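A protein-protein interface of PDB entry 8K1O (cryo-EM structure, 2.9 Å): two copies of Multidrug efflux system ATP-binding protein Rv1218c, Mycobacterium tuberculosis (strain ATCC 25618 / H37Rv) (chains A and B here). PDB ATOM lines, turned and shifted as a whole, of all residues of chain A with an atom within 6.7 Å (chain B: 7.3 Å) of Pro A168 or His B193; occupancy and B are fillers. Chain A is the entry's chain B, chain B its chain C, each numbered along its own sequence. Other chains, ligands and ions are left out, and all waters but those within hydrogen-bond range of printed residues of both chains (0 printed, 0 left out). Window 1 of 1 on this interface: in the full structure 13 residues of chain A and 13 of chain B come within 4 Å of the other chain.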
ATOM      1  N   GLY A 165       7.209   5.408  -2.138  1.00  0.00           N
ATOM      2  CA  GLY A 165       8.363   4.541  -2.152  1.00  0.00           C
ATOM      3  C   GLY A 165       9.137   4.465  -0.856  1.00  0.00           C
ATOM      4  O   GLY A 165      10.245   3.920  -0.852  1.00  0.00           O
ATOM      5  N   LEU A 166       8.593   4.986   0.238  1.00  0.00           N
ATOM      6  CA  LEU A 166       9.277   5.017   1.522  1.00  0.00           C
ATOM      7  C   LEU A 166       8.699   3.946   2.438  1.00  0.00           C
ATOM      8  O   LEU A 166       7.478   3.843   2.585  1.00  0.00           O
ATOM      9  CB  LEU A 166       9.142   6.395   2.170  1.00  0.00           C
ATOM     10  CG  LEU A 166      10.272   7.407   1.978  1.00  0.00           C
ATOM     11  CD1 LEU A 166      10.562   7.631   0.517  1.00  0.00           C
ATOM     12  CD2 LEU A 166       9.908   8.714   2.642  1.00  0.00           C
ATOM     13  N   ASP A 167       9.577   3.160   3.056  1.00  0.00           N
ATOM     14  CA  ASP A 167       9.143   2.077   3.922  1.00  0.00           C
ATOM     15  C   ASP A 167       8.505   2.641   5.191  1.00  0.00           C
ATOM     16  O   ASP A 167       8.697   3.812   5.520  1.00  0.00           O
ATOM     17  CB  ASP A 167      10.322   1.172   4.269  1.00  0.00           C
ATOM     18  CG  ASP A 167      11.447   1.915   4.928  1.00  0.00           C
ATOM     19  OD1 ASP A 167      11.622   3.102   4.610  1.00  0.00           O
ATOM     20  OD2 ASP A 167      12.156   1.320   5.765  1.00  0.00           O
ATOM     21  N   PRO A 168       7.725   1.820   5.918  1.00  0.00           N
ATOM     22  CA  PRO A 168       6.966   2.326   7.073  1.00  0.00           C
ATOM     23  C   PRO A 168       7.727   3.166   8.091  1.00  0.00           C
ATOM     24  O   PRO A 168       7.094   3.824   8.920  1.00  0.00           O
ATOM     25  CB  PRO A 168       6.456   1.036   7.721  1.00  0.00           C
ATOM     26  CG  PRO A 168       6.256   0.123   6.586  1.00  0.00           C
ATOM     27  CD  PRO A 168       7.313   0.449   5.568  1.00  0.00           C
ATOM     28  N   LEU A 169       9.059   3.162   8.064  1.00  0.00           N
ATOM     29  CA  LEU A 169       9.831   3.902   9.057  1.00  0.00           C
ATOM     30  C   LEU A 169      10.408   5.201   8.501  1.00  0.00           C
ATOM     31  O   LEU A 169      10.469   6.212   9.212  1.00  0.00           O
ATOM     32  CB  LEU A 169      10.944   3.007   9.612  1.00  0.00           C
ATOM     33  CG  LEU A 169      11.639   3.441  10.903  1.00  0.00           C
ATOM     34  CD1 LEU A 169      11.968   2.223  11.741  1.00  0.00           C
ATOM     35  CD2 LEU A 169      12.899   4.224  10.615  1.00  0.00           C
ATOM     36  N   MET A 170      10.816   5.207   7.233  1.00  0.00           N
ATOM     37  CA  MET A 170      11.278   6.437   6.604  1.00  0.00           C
ATOM     38  C   MET A 170      10.118   7.386   6.339  1.00  0.00           C
ATOM     39  O   MET A 170      10.334   8.569   6.065  1.00  0.00           O
ATOM     40  CB  MET A 170      12.014   6.145   5.296  1.00  0.00           C
ATOM     41  CG  MET A 170      13.419   5.583   5.442  1.00  0.00           C
ATOM     42  SD  MET A 170      14.434   6.451   6.650  1.00  0.00           S
ATOM     43  CE  MET A 170      14.833   5.133   7.784  1.00  0.00           C
ATOM     44  N   GLU A 171       8.889   6.890   6.418  1.00  0.00           N
ATOM     45  CA  GLU A 171       7.721   7.740   6.215  1.00  0.00           C
ATOM     46  C   GLU A 171       7.119   8.082   7.573  1.00  0.00           C
ATOM     47  O   GLU A 171       6.044   8.670   7.677  1.00  0.00           O
ATOM     48  CB  GLU A 171       6.712   7.072   5.279  1.00  0.00           C
ATOM     49  CG  GLU A 171       6.137   5.755   5.765  1.00  0.00           C
ATOM     50  CD  GLU A 171       4.930   5.926   6.663  1.00  0.00           C
ATOM     51  OE1 GLU A 171       4.303   7.004   6.622  1.00  0.00           O
ATOM     52  OE2 GLU A 171       4.604   4.980   7.411  1.00  0.00           O
ATOM     53  N   ASN A 172       7.843   7.745   8.637  1.00  0.00           N
ATOM     54  CA  ASN A 172       7.465   8.124   9.990  1.00  0.00           C
ATOM     55  C   ASN A 172       8.514   9.117  10.465  1.00  0.00           C
ATOM     56  O   ASN A 172       8.240   9.992  11.291  1.00  0.00           O
ATOM     57  CB  ASN A 172       7.389   6.886  10.886  1.00  0.00           C
ATOM     58  CG  ASN A 172       7.064   7.208  12.333  1.00  0.00           C
ATOM     59  OD1 ASN A 172       6.799   8.351  12.695  1.00  0.00           O
ATOM     60  ND2 ASN A 172       7.088   6.182  13.175  1.00  0.00           N
ATOM     61  N   VAL A 173       9.724   8.992   9.920  1.00  0.00           N
ATOM     62  CA  VAL A 173      10.723  10.047  10.078  1.00  0.00           C
ATOM     63  C   VAL A 173      10.264  11.319   9.371  1.00  0.00           C
ATOM     64  O   VAL A 173      10.435  12.434   9.883  1.00  0.00           O
ATOM     65  CB  VAL A 173      12.088   9.567   9.556  1.00  0.00           C
ATOM     66  CG1 VAL A 173      13.064  10.718   9.478  1.00  0.00           C
ATOM     67  CG2 VAL A 173      12.634   8.469  10.440  1.00  0.00           C
ATOM     68  N   PHE B  40       6.157  -9.816   0.602  1.00  0.00           N
ATOM     69  CA  PHE B  40       7.606  -9.728   0.442  1.00  0.00           C
ATOM     70  C   PHE B  40       8.013  -8.315   0.855  1.00  0.00           C
ATOM     71  O   PHE B  40       7.833  -7.366   0.089  1.00  0.00           O
ATOM     72  CB  PHE B  40       7.999 -10.057  -0.991  1.00  0.00           C
ATOM     73  CG  PHE B  40       9.475 -10.197  -1.212  1.00  0.00           C
ATOM     74  CD1 PHE B  40      10.226 -11.048  -0.426  1.00  0.00           C
ATOM     75  CD2 PHE B  40      10.096  -9.539  -2.255  1.00  0.00           C
ATOM     76  CE1 PHE B  40      11.576 -11.194  -0.639  1.00  0.00           C
ATOM     77  CE2 PHE B  40      11.443  -9.688  -2.474  1.00  0.00           C
ATOM     78  CZ  PHE B  40      12.184 -10.515  -1.666  1.00  0.00           C
ATOM     79  N   LEU B  41       8.557  -8.190   2.064  1.00  0.00           N
ATOM     80  CA  LEU B  41       8.722  -6.912   2.736  1.00  0.00           C
ATOM     81  C   LEU B  41      10.192  -6.646   3.037  1.00  0.00           C
ATOM     82  O   LEU B  41      11.043  -7.526   2.901  1.00  0.00           O
ATOM     83  CB  LEU B  41       7.917  -6.882   4.040  1.00  0.00           C
ATOM     84  CG  LEU B  41       6.451  -7.299   3.942  1.00  0.00           C
ATOM     85  CD1 LEU B  41       5.831  -7.386   5.320  1.00  0.00           C
ATOM     86  CD2 LEU B  41       5.678  -6.329   3.077  1.00  0.00           C
ATOM     87  N   GLY B  42      10.481  -5.415   3.461  1.00  0.00           N
ATOM     88  CA  GLY B  42      11.822  -5.030   3.837  1.00  0.00           C
ATOM     89  C   GLY B  42      12.107  -3.556   3.621  1.00  0.00           C
ATOM     90  O   GLY B  42      11.402  -2.865   2.883  1.00  0.00           O
ATOM     91  N   PRO B  43      13.165  -3.047   4.262  1.00  0.00           N
ATOM     92  CA  PRO B  43      13.510  -1.623   4.122  1.00  0.00           C
ATOM     93  C   PRO B  43      14.003  -1.266   2.729  1.00  0.00           C
ATOM     94  O   PRO B  43      13.998  -2.116   1.836  1.00  0.00           O
ATOM     95  CB  PRO B  43      14.614  -1.422   5.168  1.00  0.00           C
ATOM     96  CG  PRO B  43      15.073  -2.783   5.535  1.00  0.00           C
ATOM     97  CD  PRO B  43      13.915  -3.692   5.350  1.00  0.00           C
ATOM     98  N   ASN B  44      14.420  -0.017   2.519  1.00  0.00           N
ATOM     99  CA  ASN B  44      14.851   0.414   1.188  1.00  0.00           C
ATOM    100  C   ASN B  44      16.213  -0.008   0.666  1.00  0.00           C
ATOM    101  O   ASN B  44      16.630   0.429  -0.408  1.00  0.00           O
ATOM    102  CB  ASN B  44      14.580   1.907   1.023  1.00  0.00           C
ATOM    103  CG  ASN B  44      13.118   2.248   1.084  1.00  0.00           C
ATOM    104  OD1 ASN B  44      12.668   2.933   1.998  1.00  0.00           O
ATOM    105  ND2 ASN B  44      12.362   1.786   0.100  1.00  0.00           N
ATOM    106  N   GLY B  45      16.925  -0.871   1.380  1.00  0.00           N
ATOM    107  CA  GLY B  45      18.110  -1.506   0.846  1.00  0.00           C
ATOM    108  C   GLY B  45      18.089  -3.000   0.628  1.00  0.00           C
ATOM    109  O   GLY B  45      19.065  -3.590   0.159  1.00  0.00           O
ATOM    110  N   LYS B  48      14.648  -6.211  -2.805  1.00  0.00           N
ATOM    111  CA  LYS B  48      13.367  -6.739  -3.258  1.00  0.00           C
ATOM    112  C   LYS B  48      13.203  -6.593  -4.764  1.00  0.00           C
ATOM    113  O   LYS B  48      12.720  -7.513  -5.431  1.00  0.00           O
ATOM    114  CB  LYS B  48      12.226  -6.034  -2.531  1.00  0.00           C
ATOM    115  CG  LYS B  48      12.291  -6.130  -1.024  1.00  0.00           C
ATOM    116  CD  LYS B  48      11.095  -5.456  -0.395  1.00  0.00           C
ATOM    117  CE  LYS B  48      11.025  -4.000  -0.787  1.00  0.00           C
ATOM    118  NZ  LYS B  48      12.045  -3.195  -0.072  1.00  0.00           N
ATOM    119  N   SER B  49      13.585  -5.444  -5.318  1.00  0.00           N
ATOM    120  CA  SER B  49      13.447  -5.249  -6.756  1.00  0.00           C
ATOM    121  C   SER B  49      14.502  -6.021  -7.529  1.00  0.00           C
ATOM    122  O   SER B  49      14.278  -6.375  -8.690  1.00  0.00           O
ATOM    123  CB  SER B  49      13.527  -3.765  -7.100  1.00  0.00           C
ATOM    124  OG  SER B  49      12.638  -3.008  -6.300  1.00  0.00           O
ATOM    125  N   ASP B 160       5.558  -5.647  -8.088  1.00  0.00           N
ATOM    126  CA  ASP B 160       6.592  -4.906  -7.376  1.00  0.00           C
ATOM    127  C   ASP B 160       6.018  -3.792  -6.515  1.00  0.00           C
ATOM    128  O   ASP B 160       6.459  -3.597  -5.379  1.00  0.00           O
ATOM    129  CB  ASP B 160       7.596  -4.323  -8.368  1.00  0.00           C
ATOM    130  CG  ASP B 160       8.987  -4.214  -7.791  1.00  0.00           C
ATOM    131  OD1 ASP B 160       9.115  -4.147  -6.552  1.00  0.00           O
ATOM    132  OD2 ASP B 160       9.957  -4.195  -8.579  1.00  0.00           O
ATOM    133  N   GLU B 161       5.062  -3.046  -7.038  1.00  0.00           N
ATOM    134  CA  GLU B 161       4.327  -2.052  -6.272  1.00  0.00           C
ATOM    135  C   GLU B 161       3.044  -1.776  -7.042  1.00  0.00           C
ATOM    136  O   GLU B 161       2.912  -0.729  -7.688  1.00  0.00           O
ATOM    137  CB  GLU B 161       5.147  -0.780  -6.075  1.00  0.00           C
ATOM    138  CG  GLU B 161       4.467   0.270  -5.218  1.00  0.00           C
ATOM    139  CD  GLU B 161       4.364  -0.154  -3.771  1.00  0.00           C
ATOM    140  OE1 GLU B 161       5.256  -0.898  -3.317  1.00  0.00           O
ATOM    141  OE2 GLU B 161       3.398   0.252  -3.092  1.00  0.00           O
ATOM    142  N   LEU B 190       3.923 -10.359  -3.883  1.00  0.00           N
ATOM    143  CA  LEU B 190       3.556  -8.953  -3.770  1.00  0.00           C
ATOM    144  C   LEU B 190       4.568  -8.213  -2.904  1.00  0.00           C
ATOM    145  O   LEU B 190       4.830  -8.625  -1.770  1.00  0.00           O
ATOM    146  CB  LEU B 190       2.155  -8.837  -3.167  1.00  0.00           C
ATOM    147  CG  LEU B 190       1.455  -7.488  -3.074  1.00  0.00           C
ATOM    148  CD1 LEU B 190       0.705  -7.212  -4.348  1.00  0.00           C
ATOM    149  CD2 LEU B 190       0.510  -7.474  -1.889  1.00  0.00           C
ATOM    150  N   SER B 191       5.124  -7.122  -3.430  1.00  0.00           N
ATOM    151  CA  SER B 191       5.961  -6.213  -2.652  1.00  0.00           C
ATOM    152  C   SER B 191       5.198  -4.915  -2.431  1.00  0.00           C
ATOM    153  O   SER B 191       4.730  -4.301  -3.394  1.00  0.00           O
ATOM    154  CB  SER B 191       7.287  -5.937  -3.364  1.00  0.00           C
ATOM    155  OG  SER B 191       7.909  -7.141  -3.769  1.00  0.00           O
ATOM    156  N   SER B 192       5.059  -4.501  -1.171  1.00  0.00           N
ATOM    157  CA  SER B 192       4.062  -3.487  -0.845  1.00  0.00           C
ATOM    158  C   SER B 192       4.622  -2.200  -0.252  1.00  0.00           C
ATOM    159  O   SER B 192       4.318  -1.118  -0.764  1.00  0.00           O
ATOM    160  CB  SER B 192       3.026  -4.089   0.114  1.00  0.00           C
ATOM    161  OG  SER B 192       1.970  -3.179   0.355  1.00  0.00           O
ATOM    162  N   HIS B 193       5.402  -2.278   0.832  1.00  0.00           N
ATOM    163  CA  HIS B 193       5.661  -1.140   1.721  1.00  0.00           C
ATOM    164  C   HIS B 193       4.388  -0.589   2.354  1.00  0.00           C
ATOM    165  O   HIS B 193       4.442   0.401   3.089  1.00  0.00           O
ATOM    166  CB  HIS B 193       6.397   0.015   1.028  1.00  0.00           C
ATOM    167  CG  HIS B 193       7.802  -0.299   0.625  1.00  0.00           C
ATOM    168  ND1 HIS B 193       8.822  -0.417   1.544  1.00  0.00           N
ATOM    169  CD2 HIS B 193       8.370  -0.460  -0.591  1.00  0.00           C
ATOM    170  CE1 HIS B 193       9.954  -0.670   0.911  1.00  0.00           C
ATOM    171  NE2 HIS B 193       9.707  -0.700  -0.385  1.00  0.00           N
ATOM    172  N   ILE B 194       3.246  -1.209   2.085  1.00  0.00           N
ATOM    173  CA  ILE B 194       1.967  -0.800   2.648  1.00  0.00           C
ATOM    174  C   ILE B 194       1.453  -1.988   3.448  1.00  0.00           C
ATOM    175  O   ILE B 194       0.934  -2.955   2.880  1.00  0.00           O
ATOM    176  CB  ILE B 194       0.961  -0.374   1.574  1.00  0.00           C
ATOM    177  CG1 ILE B 194       1.448   0.884   0.857  1.00  0.00           C
ATOM    178  CG2 ILE B 194      -0.397  -0.120   2.192  1.00  0.00           C
ATOM    179  CD1 ILE B 194       0.568   1.304  -0.292  1.00  0.00           C
ATOM    180  N   LEU B 195       1.596  -1.924   4.767  1.00  0.00           N
ATOM    181  CA  LEU B 195       1.205  -3.025   5.634  1.00  0.00           C
ATOM    182  C   LEU B 195      -0.283  -3.033   5.942  1.00  0.00           C
ATOM    183  O   LEU B 195      -0.709  -3.708   6.883  1.00  0.00           O
ATOM    184  CB  LEU B 195       2.018  -2.980   6.929  1.00  0.00           C
ATOM    185  CG  LEU B 195       3.534  -2.885   6.743  1.00  0.00           C
ATOM    186  CD1 LEU B 195       4.248  -3.059   8.065  1.00  0.00           C
ATOM    187  CD2 LEU B 195       4.025  -3.908   5.737  1.00  0.00           C
ATOM    188  N   ALA B 196      -1.080  -2.294   5.173  1.00  0.00           N
ATOM    189  CA  ALA B 196      -2.532  -2.303   5.299  1.00  0.00           C
ATOM    190  C   ALA B 196      -3.192  -3.191   4.254  1.00  0.00           C
ATOM    191  O   ALA B 196      -4.222  -3.809   4.529  1.00  0.00           O
ATOM    192  CB  ALA B 196      -3.080  -0.875   5.198  1.00  0.00           C
ATOM    193  N   GLU B 197      -2.622  -3.255   3.049  1.00  0.00           N
ATOM    194  CA  GLU B 197      -3.102  -4.210   2.057  1.00  0.00           C
ATOM    195  C   GLU B 197      -2.440  -5.570   2.231  1.00  0.00           C
ATOM    196  O   GLU B 197      -3.036  -6.595   1.889  1.00  0.00           O
ATOM    197  CB  GLU B 197      -2.872  -3.671   0.646  1.00  0.00           C
ATOM    198  CG  GLU B 197      -1.437  -3.753   0.161  1.00  0.00           C
ATOM    199  CD  GLU B 197      -1.286  -3.336  -1.288  1.00  0.00           C
ATOM    200  OE1 GLU B 197      -2.317  -3.072  -1.941  1.00  0.00           O
ATOM    201  OE2 GLU B 197      -0.137  -3.270  -1.776  1.00  0.00           O
ATOM    202  N   THR B 198      -1.215  -5.597   2.758  1.00  0.00           N
ATOM    203  CA  THR B 198      -0.567  -6.866   3.073  1.00  0.00           C
ATOM    204  C   THR B 198      -1.345  -7.629   4.135  1.00  0.00           C
ATOM    205  O   THR B 198      -1.493  -8.854   4.051  1.00  0.00           O
ATOM    206  CB  THR B 198       0.868  -6.616   3.534  1.00  0.00           C
ATOM    207  OG1 THR B 198       1.613  -6.004   2.475  1.00  0.00           O
ATOM    208  CG2 THR B 198       1.538  -7.911   3.941  1.00  0.00           C
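The backbone NH of Met A170 sits close to the side-chain carboxylate of Asp A167 (3.5 Å).
The backbone carbonyl oxygen (O) of Pro B43 sits at hydrogen-bond distance from the side-chain amino group (NZ) of Lys B48 (2.9 Å).
NZ of Lys B48 sits close to NE2 of His B193, 3.4 Å away.
Pro B43 touches Asp A167.
CA of Asp A167 touches ND1 of His B193 (3.5 Å).
Pro A168 touches His B193 (CD to O, 3.8 Å).
The side-chain amide nitrogen (ND2) of Asn B44 sits at hydrogen-bond distance from the backbone carbonyl oxygen (O) of Gly A165 (3.2 Å).
The side-chain carboxylate (OD1) of Asp A167 lies close to the side-chain amide oxygen (OD1) of Asn B44 (2.8 Å).
No position is printed for both chains.
Hydrophobic or aromatic side chains of chain A that line the printed part of chain B: Pro A168.
Along chain A the printed residues that touch a printed residue of chain B span positions 165 to 168.
Among the printed residues, 5 pairs touch across the chains.
Among the printed residues, no Asp or Glu carboxylate lies within 4 Å of a Lys or Arg side-chain nitrogen of the other chain.
Of the printed residues of chain B, Gly A165 touches Asn B44.
Leu A166 touches none of the printed residues of chain B.
Pro A168 touches just one residue of chain B: His B193 (3.8 Å).
Of the printed residues of chain A, Pro B43 touches Asp A167 (3.6 Å).
Printed residues of chain A within 4 Å of Asn B44: Gly A165 and Asp A167.
Ala B196 touches none of the printed residues of chain A.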
